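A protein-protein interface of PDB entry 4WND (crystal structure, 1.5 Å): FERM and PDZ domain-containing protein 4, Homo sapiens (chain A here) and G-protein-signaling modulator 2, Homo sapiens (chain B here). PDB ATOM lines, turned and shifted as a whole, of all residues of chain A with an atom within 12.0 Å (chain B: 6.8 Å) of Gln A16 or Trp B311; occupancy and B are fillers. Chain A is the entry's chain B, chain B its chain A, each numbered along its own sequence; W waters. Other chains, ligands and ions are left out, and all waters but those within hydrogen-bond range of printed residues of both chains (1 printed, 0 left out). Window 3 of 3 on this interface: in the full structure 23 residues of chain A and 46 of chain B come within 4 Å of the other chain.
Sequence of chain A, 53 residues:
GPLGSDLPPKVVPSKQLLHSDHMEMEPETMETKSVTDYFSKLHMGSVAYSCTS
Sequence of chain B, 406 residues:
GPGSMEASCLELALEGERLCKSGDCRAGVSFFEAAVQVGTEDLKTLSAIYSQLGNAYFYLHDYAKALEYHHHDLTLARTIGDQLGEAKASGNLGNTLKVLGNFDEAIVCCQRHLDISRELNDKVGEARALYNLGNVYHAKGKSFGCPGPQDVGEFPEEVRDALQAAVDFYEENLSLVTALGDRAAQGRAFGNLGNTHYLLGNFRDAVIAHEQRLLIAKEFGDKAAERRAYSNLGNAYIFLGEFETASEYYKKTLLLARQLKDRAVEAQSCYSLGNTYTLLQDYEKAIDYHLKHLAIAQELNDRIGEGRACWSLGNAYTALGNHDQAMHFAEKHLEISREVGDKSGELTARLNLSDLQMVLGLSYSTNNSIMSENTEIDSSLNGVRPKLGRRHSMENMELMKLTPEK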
ATOM      1  N   GLN A  16      -1.855  22.231   6.518  1.00  0.00           N
ATOM      2  CA  GLN A  16      -1.153  21.026   5.975  1.00  0.00           C
ATOM      3  C   GLN A  16      -2.053  19.784   6.006  1.00  0.00           C
ATOM      4  O   GLN A  16      -2.074  18.998   5.050  1.00  0.00           O
ATOM      5  CB  GLN A  16       0.133  20.755   6.769  1.00  0.00           C
ATOM      6  N   LEU A  17      -2.803  19.627   7.101  1.00  0.00           N
ATOM      7  CA  LEU A  17      -3.553  18.390   7.376  1.00  0.00           C
ATOM      8  C   LEU A  17      -4.985  18.415   6.847  1.00  0.00           C
ATOM      9  O   LEU A  17      -5.674  19.432   6.931  1.00  0.00           O
ATOM     10  CB  LEU A  17      -3.601  18.118   8.892  1.00  0.00           C
ATOM     11  CG  LEU A  17      -2.353  17.517   9.547  1.00  0.00           C
ATOM     12  CD1 LEU A  17      -2.670  17.119  10.976  1.00  0.00           C
ATOM     13  CD2 LEU A  17      -1.835  16.318   8.761  1.00  0.00           C
ATOM     14  N   LEU A  18      -5.430  17.275   6.322  1.00  0.00           N
ATOM     15  CA  LEU A  18      -6.845  17.046   6.074  1.00  0.00           C
ATOM     16  C   LEU A  18      -7.407  16.211   7.218  1.00  0.00           C
ATOM     17  O   LEU A  18      -7.242  14.999   7.240  1.00  0.00           O
ATOM     18  CB  LEU A  18      -7.052  16.310   4.748  1.00  0.00           C
ATOM     19  CG  LEU A  18      -6.547  16.994   3.482  1.00  0.00           C
ATOM     20  CD1 LEU A  18      -6.839  16.105   2.274  1.00  0.00           C
ATOM     21  CD2 LEU A  18      -7.169  18.382   3.322  1.00  0.00           C
ATOM     22  N   HIS A  19      -8.042  16.870   8.184  1.00  0.00           N
ATOM     23  CA  HIS A  19      -8.698  16.165   9.288  1.00  0.00           C
ATOM     24  C   HIS A  19      -9.959  15.475   8.782  1.00  0.00           C
ATOM     25  O   HIS A  19     -10.656  16.005   7.910  1.00  0.00           O
ATOM     26  CB  HIS A  19      -9.052  17.137  10.419  1.00  0.00           C
ATOM     27  CG  HIS A  19      -7.869  17.595  11.211  1.00  0.00           C
ATOM     28  ND1 HIS A  19      -7.531  17.044  12.428  1.00  0.00           N
ATOM     29  CD2 HIS A  19      -6.938  18.543  10.954  1.00  0.00           C
ATOM     30  CE1 HIS A  19      -6.445  17.638  12.891  1.00  0.00           C
ATOM     31  NE2 HIS A  19      -6.064  18.552  12.014  1.00  0.00           N
ATOM     32  N   SER A  20     -10.238  14.285   9.314  1.00  0.00           N
ATOM     33  CA  SER A  20     -11.453  13.545   8.951  1.00  0.00           C
ATOM     34  C   SER A  20     -12.628  13.971   9.835  1.00  0.00           C
ATOM     35  O   SER A  20     -12.434  14.458  10.956  1.00  0.00           O
ATOM     36  CB  SER A  20     -11.223  12.036   9.066  1.00  0.00           C
ATOM     37  OG  SER A  20     -10.787  11.687  10.367  1.00  0.00           O
ATOM     38  N   TYR B 271      -6.071   6.553   9.926  1.00  0.00           N
ATOM     39  CA  TYR B 271      -5.987   7.898   9.355  1.00  0.00           C
ATOM     40  C   TYR B 271      -5.748   8.916  10.472  1.00  0.00           C
ATOM     41  O   TYR B 271      -4.875   9.789  10.366  1.00  0.00           O
ATOM     42  CB  TYR B 271      -7.263   8.211   8.574  1.00  0.00           C
ATOM     43  CG  TYR B 271      -7.150   9.477   7.773  1.00  0.00           C
ATOM     44  CD1 TYR B 271      -6.584   9.463   6.503  1.00  0.00           C
ATOM     45  CD2 TYR B 271      -7.577  10.681   8.293  1.00  0.00           C
ATOM     46  CE1 TYR B 271      -6.453  10.634   5.774  1.00  0.00           C
ATOM     47  CE2 TYR B 271      -7.455  11.849   7.567  1.00  0.00           C
ATOM     48  CZ  TYR B 271      -6.886  11.813   6.318  1.00  0.00           C
ATOM     49  OH  TYR B 271      -6.758  12.974   5.595  1.00  0.00           O
ATOM     50  N   THR B 278       1.780  13.140  12.183  1.00  0.00           N
ATOM     51  CA  THR B 278       2.155  14.331  11.415  1.00  0.00           C
ATOM     52  C   THR B 278       2.247  15.542  12.339  1.00  0.00           C
ATOM     53  O   THR B 278       3.213  16.304  12.271  1.00  0.00           O
ATOM     54  CB  THR B 278       1.170  14.594  10.270  1.00  0.00           C
ATOM     55  OG1 THR B 278       1.319  13.567   9.289  1.00  0.00           O
ATOM     56  CG2 THR B 278       1.402  15.993   9.629  1.00  0.00           C
ATOM     57  N   GLU B 306      -9.293   7.313  -0.487  1.00  0.00           N
ATOM     58  CA  GLU B 306      -8.033   7.074  -1.210  1.00  0.00           C
ATOM     59  C   GLU B 306      -7.362   8.401  -1.590  1.00  0.00           C
ATOM     60  O   GLU B 306      -6.156   8.550  -1.441  1.00  0.00           O
ATOM     61  CB  GLU B 306      -8.248   6.231  -2.466  1.00  0.00           C
ATOM     62  CG  GLU B 306      -6.949   5.846  -3.171  1.00  0.00           C
ATOM     63  CD  GLU B 306      -7.141   4.810  -4.275  1.00  0.00           C
ATOM     64  OE1 GLU B 306      -6.118   4.319  -4.820  1.00  0.00           O
ATOM     65  OE2 GLU B 306      -8.304   4.464  -4.572  1.00  0.00           O
ATOM     66  N   GLY B 307      -8.135   9.367  -2.046  1.00  0.00           N
ATOM     67  CA  GLY B 307      -7.557  10.666  -2.375  1.00  0.00           C
ATOM     68  C   GLY B 307      -6.933  11.382  -1.191  1.00  0.00           C
ATOM     69  O   GLY B 307      -5.855  11.976  -1.314  1.00  0.00           O
ATOM     70  N   ARG B 308      -7.606  11.339  -0.048  1.00  0.00           N
ATOM     71  CA  ARG B 308      -7.138  12.011   1.142  1.00  0.00           C
ATOM     72  C   ARG B 308      -5.879  11.323   1.659  1.00  0.00           C
ATOM     73  O   ARG B 308      -4.976  11.980   2.166  1.00  0.00           O
ATOM     74  CB  ARG B 308      -8.234  12.000   2.201  1.00  0.00           C
ATOM     75  CG  ARG B 308      -9.502  12.717   1.744  1.00  0.00           C
ATOM     76  CD  ARG B 308     -10.692  12.339   2.605  1.00  0.00           C
ATOM     77  NE  ARG B 308     -10.471  12.717   3.996  1.00  0.00           N
ATOM     78  CZ  ARG B 308     -10.628  13.948   4.470  1.00  0.00           C
ATOM     79  NH1 ARG B 308     -11.012  14.926   3.661  1.00  0.00           N
ATOM     80  NH2 ARG B 308     -10.406  14.202   5.751  1.00  0.00           N
ATOM     81  N   ALA B 309      -5.848  10.003   1.528  1.00  0.00           N
ATOM     82  CA  ALA B 309      -4.654   9.193   1.844  1.00  0.00           C
ATOM     83  C   ALA B 309      -3.475   9.626   0.983  1.00  0.00           C
ATOM     84  O   ALA B 309      -2.363   9.828   1.487  1.00  0.00           O
ATOM     85  CB  ALA B 309      -4.935   7.733   1.612  1.00  0.00           C
ATOM     86  N   CYS B 310      -3.710   9.769  -0.328  1.00  0.00           N
ATOM     87  CA  CYS B 310      -2.603  10.146  -1.241  1.00  0.00           C
ATOM     88  C   CYS B 310      -2.056  11.543  -0.880  1.00  0.00           C
ATOM     89  O   CYS B 310      -0.821  11.776  -0.878  1.00  0.00           O
ATOM     90  CB  CYS B 310      -3.052  10.107  -2.700  1.00  0.00           C
ATOM     91  SG  CYS B 310      -3.429   8.468  -3.317  1.00  0.00           S
ATOM     92  N   TRP B 311      -2.943  12.470  -0.546  1.00  0.00           N
ATOM     93  CA  TRP B 311      -2.503  13.792  -0.093  1.00  0.00           C
ATOM     94  C   TRP B 311      -1.685  13.696   1.182  1.00  0.00           C
ATOM     95  O   TRP B 311      -0.599  14.255   1.286  1.00  0.00           O
ATOM     96  CB  TRP B 311      -3.694  14.729   0.135  1.00  0.00           C
ATOM     97  CG  TRP B 311      -3.281  16.109   0.489  1.00  0.00           C
ATOM     98  CD1 TRP B 311      -3.190  16.633   1.738  1.00  0.00           C
ATOM     99  CD2 TRP B 311      -2.859  17.139  -0.416  1.00  0.00           C
ATOM    100  NE1 TRP B 311      -2.770  17.945   1.674  1.00  0.00           N
ATOM    101  CE2 TRP B 311      -2.547  18.272   0.361  1.00  0.00           C
ATOM    102  CE3 TRP B 311      -2.735  17.216  -1.797  1.00  0.00           C
ATOM    103  CZ2 TRP B 311      -2.127  19.480  -0.211  1.00  0.00           C
ATOM    104  CZ3 TRP B 311      -2.298  18.406  -2.369  1.00  0.00           C
ATOM    105  CH2 TRP B 311      -1.991  19.517  -1.578  1.00  0.00           C
ATOM    106  N   SER B 312      -2.182  12.929   2.153  1.00  0.00           N
ATOM    107  CA  SER B 312      -1.505  12.832   3.419  1.00  0.00           C
ATOM    108  C   SER B 312      -0.128  12.146   3.282  1.00  0.00           C
ATOM    109  O   SER B 312       0.835  12.589   3.868  1.00  0.00           O
ATOM    110  CB  SER B 312      -2.357  12.048   4.389  1.00  0.00           C
ATOM    111  OG  SER B 312      -3.575  12.751   4.653  1.00  0.00           O
ATOM    112  N   LEU B 313      -0.074  11.118   2.460  1.00  0.00           N
ATOM    113  CA  LEU B 313       1.179  10.408   2.205  1.00  0.00           C
ATOM    114  C   LEU B 313       2.168  11.285   1.461  1.00  0.00           C
ATOM    115  O   LEU B 313       3.331  11.378   1.829  1.00  0.00           O
ATOM    116  CB  LEU B 313       0.931   9.134   1.415  1.00  0.00           C
ATOM    117  CG  LEU B 313       0.311   8.024   2.259  1.00  0.00           C
ATOM    118  CD1 LEU B 313      -0.337   6.950   1.405  1.00  0.00           C
ATOM    119  CD2 LEU B 313       1.400   7.410   3.133  1.00  0.00           C
ATOM    120  N   GLY B 314       1.699  11.988   0.451  1.00  0.00           N
ATOM    121  CA  GLY B 314       2.602  12.895  -0.273  1.00  0.00           C
ATOM    122  C   GLY B 314       3.196  13.966   0.599  1.00  0.00           C
ATOM    123  O   GLY B 314       4.383  14.278   0.483  1.00  0.00           O
ATOM    124  N   ASN B 315       2.368  14.535   1.480  1.00  0.00           N
ATOM    125  CA  ASN B 315       2.832  15.559   2.408  1.00  0.00           C
ATOM    126  C   ASN B 315       3.900  14.996   3.326  1.00  0.00           C
ATOM    127  O   ASN B 315       4.949  15.628   3.527  1.00  0.00           O
ATOM    128  CB  ASN B 315       1.670  16.139   3.223  1.00  0.00           C
ATOM    129  CG  ASN B 315       1.016  17.311   2.537  1.00  0.00           C
ATOM    130  OD1 ASN B 315      -0.078  17.196   1.993  1.00  0.00           O
ATOM    131  ND2 ASN B 315       1.684  18.435   2.547  1.00  0.00           N
ATOM    132  N   ALA B 316       3.658  13.804   3.874  1.00  0.00           N
ATOM    133  CA  ALA B 316       4.610  13.195   4.805  1.00  0.00           C
ATOM    134  C   ALA B 316       5.922  12.792   4.120  1.00  0.00           C
ATOM    135  O   ALA B 316       7.000  13.080   4.630  1.00  0.00           O
ATOM    136  CB  ALA B 316       3.975  11.994   5.503  1.00  0.00           C
ATOM    137  N   PHE B 329       2.538   9.700  -5.115  1.00  0.00           N
ATOM    138  CA  PHE B 329       1.248  10.000  -4.530  1.00  0.00           C
ATOM    139  C   PHE B 329       0.655  11.309  -5.055  1.00  0.00           C
ATOM    140  O   PHE B 329      -0.571  11.463  -5.052  1.00  0.00           O
ATOM    141  CB  PHE B 329       1.295   9.948  -3.006  1.00  0.00           C
ATOM    142  CG  PHE B 329       1.417   8.565  -2.496  1.00  0.00           C
ATOM    143  CD1 PHE B 329       0.338   7.694  -2.625  1.00  0.00           C
ATOM    144  CD2 PHE B 329       2.625   8.066  -2.019  1.00  0.00           C
ATOM    145  CE1 PHE B 329       0.454   6.365  -2.234  1.00  0.00           C
ATOM    146  CE2 PHE B 329       2.743   6.730  -1.645  1.00  0.00           C
ATOM    147  CZ  PHE B 329       1.643   5.895  -1.734  1.00  0.00           C
ATOM    148  N   ALA B 330       1.492  12.239  -5.526  1.00  0.00           N
ATOM    149  CA  ALA B 330       0.973  13.447  -6.187  1.00  0.00           C
ATOM    150  C   ALA B 330       0.198  13.055  -7.441  1.00  0.00           C
ATOM    151  O   ALA B 330      -0.890  13.593  -7.699  1.00  0.00           O
ATOM    152  CB  ALA B 330       2.100  14.422  -6.549  1.00  0.00           C
ATOM    153  N   HIS B 333      -2.990  11.445  -6.424  1.00  0.00           N
ATOM    154  CA  HIS B 333      -3.885  12.454  -5.897  1.00  0.00           C
ATOM    155  C   HIS B 333      -4.528  13.253  -7.018  1.00  0.00           C
ATOM    156  O   HIS B 333      -5.745  13.459  -7.007  1.00  0.00           O
ATOM    157  CB  HIS B 333      -3.176  13.392  -4.936  1.00  0.00           C
ATOM    158  CG  HIS B 333      -4.039  14.505  -4.458  1.00  0.00           C
ATOM    159  ND1 HIS B 333      -3.988  15.772  -4.993  1.00  0.00           N
ATOM    160  CD2 HIS B 333      -5.009  14.533  -3.515  1.00  0.00           C
ATOM    161  CE1 HIS B 333      -4.874  16.542  -4.378  1.00  0.00           C
ATOM    162  NE2 HIS B 333      -5.495  15.813  -3.469  1.00  0.00           N
HETATM  163  O   HOH W   1      -3.732  14.749   6.369  1.00  0.00           O
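NE1 of Trp B311 touches O of Gln A16, at 3.6 Å.
Leu A17 touches Thr B278 (CD2 to CG2, 3.4 Å).
O of Leu A18 touches NH2 of Arg B308, 3.6 Å away.
Leu A18 touches Trp B311.
Ser A20 touches Tyr B271.
CA of Ser A20 touches NH2 of Arg B308 (3.4 Å).
Water W1 lies within hydrogen-bond range of OG of Ser B312 and N of Leu A18.
Printed residues of chain A that touch a printed residue of chain B: Gln A16, Leu A17, Leu A18, His A19 and Ser A20.
Hydrophobic or aromatic side chains of chain A within 4 Å of the printed part of chain B: Leu A17 and Leu A18.
OD1 of Asn B315 lies within hydrogen-bond range of NE1 of Trp B311 (2.8 Å).
The side-chain hydroxyl (OG) of Ser B312 lies within hydrogen-bond range of the side-chain hydroxyl (OH) of Tyr B271.
The backbone carbonyl oxygen (O) of Arg B308 is in hydrogen-bond range of the side-chain hydroxyl (OG) of Ser B312, at 3.0 Å.
The side-chain hydroxyl (OH) of Tyr B271 is in hydrogen-bond range of the backbone carbonyl oxygen (O) of Leu A18 (2.7 Å).
The backbone carbonyl oxygen (O) of His A19 lies within hydrogen-bond range of the guanidinium group (NH2) of Arg B308.
Gln A16 touches one residue of chain B.
Of chain A, only Gln A16 (3.6 Å) and Leu A18 (3.7 Å) come within 4 Å of Trp B311.
No residue of chain A comes within 4 Å of Ala B309.
No residue of chain A comes within 4 Å of Cys B310.
No residue of chain A comes within 4 Å of Ser B312.
No residue of chain A comes within 4 Å of Gly B314.
Of the printed residues of chain B, Ser A20 touches Tyr B271 and Arg B308.
Of the printed residues of chain A, Tyr B271 touches Leu A18 (2.7 Å) and Ser A20 (3.95 Å).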
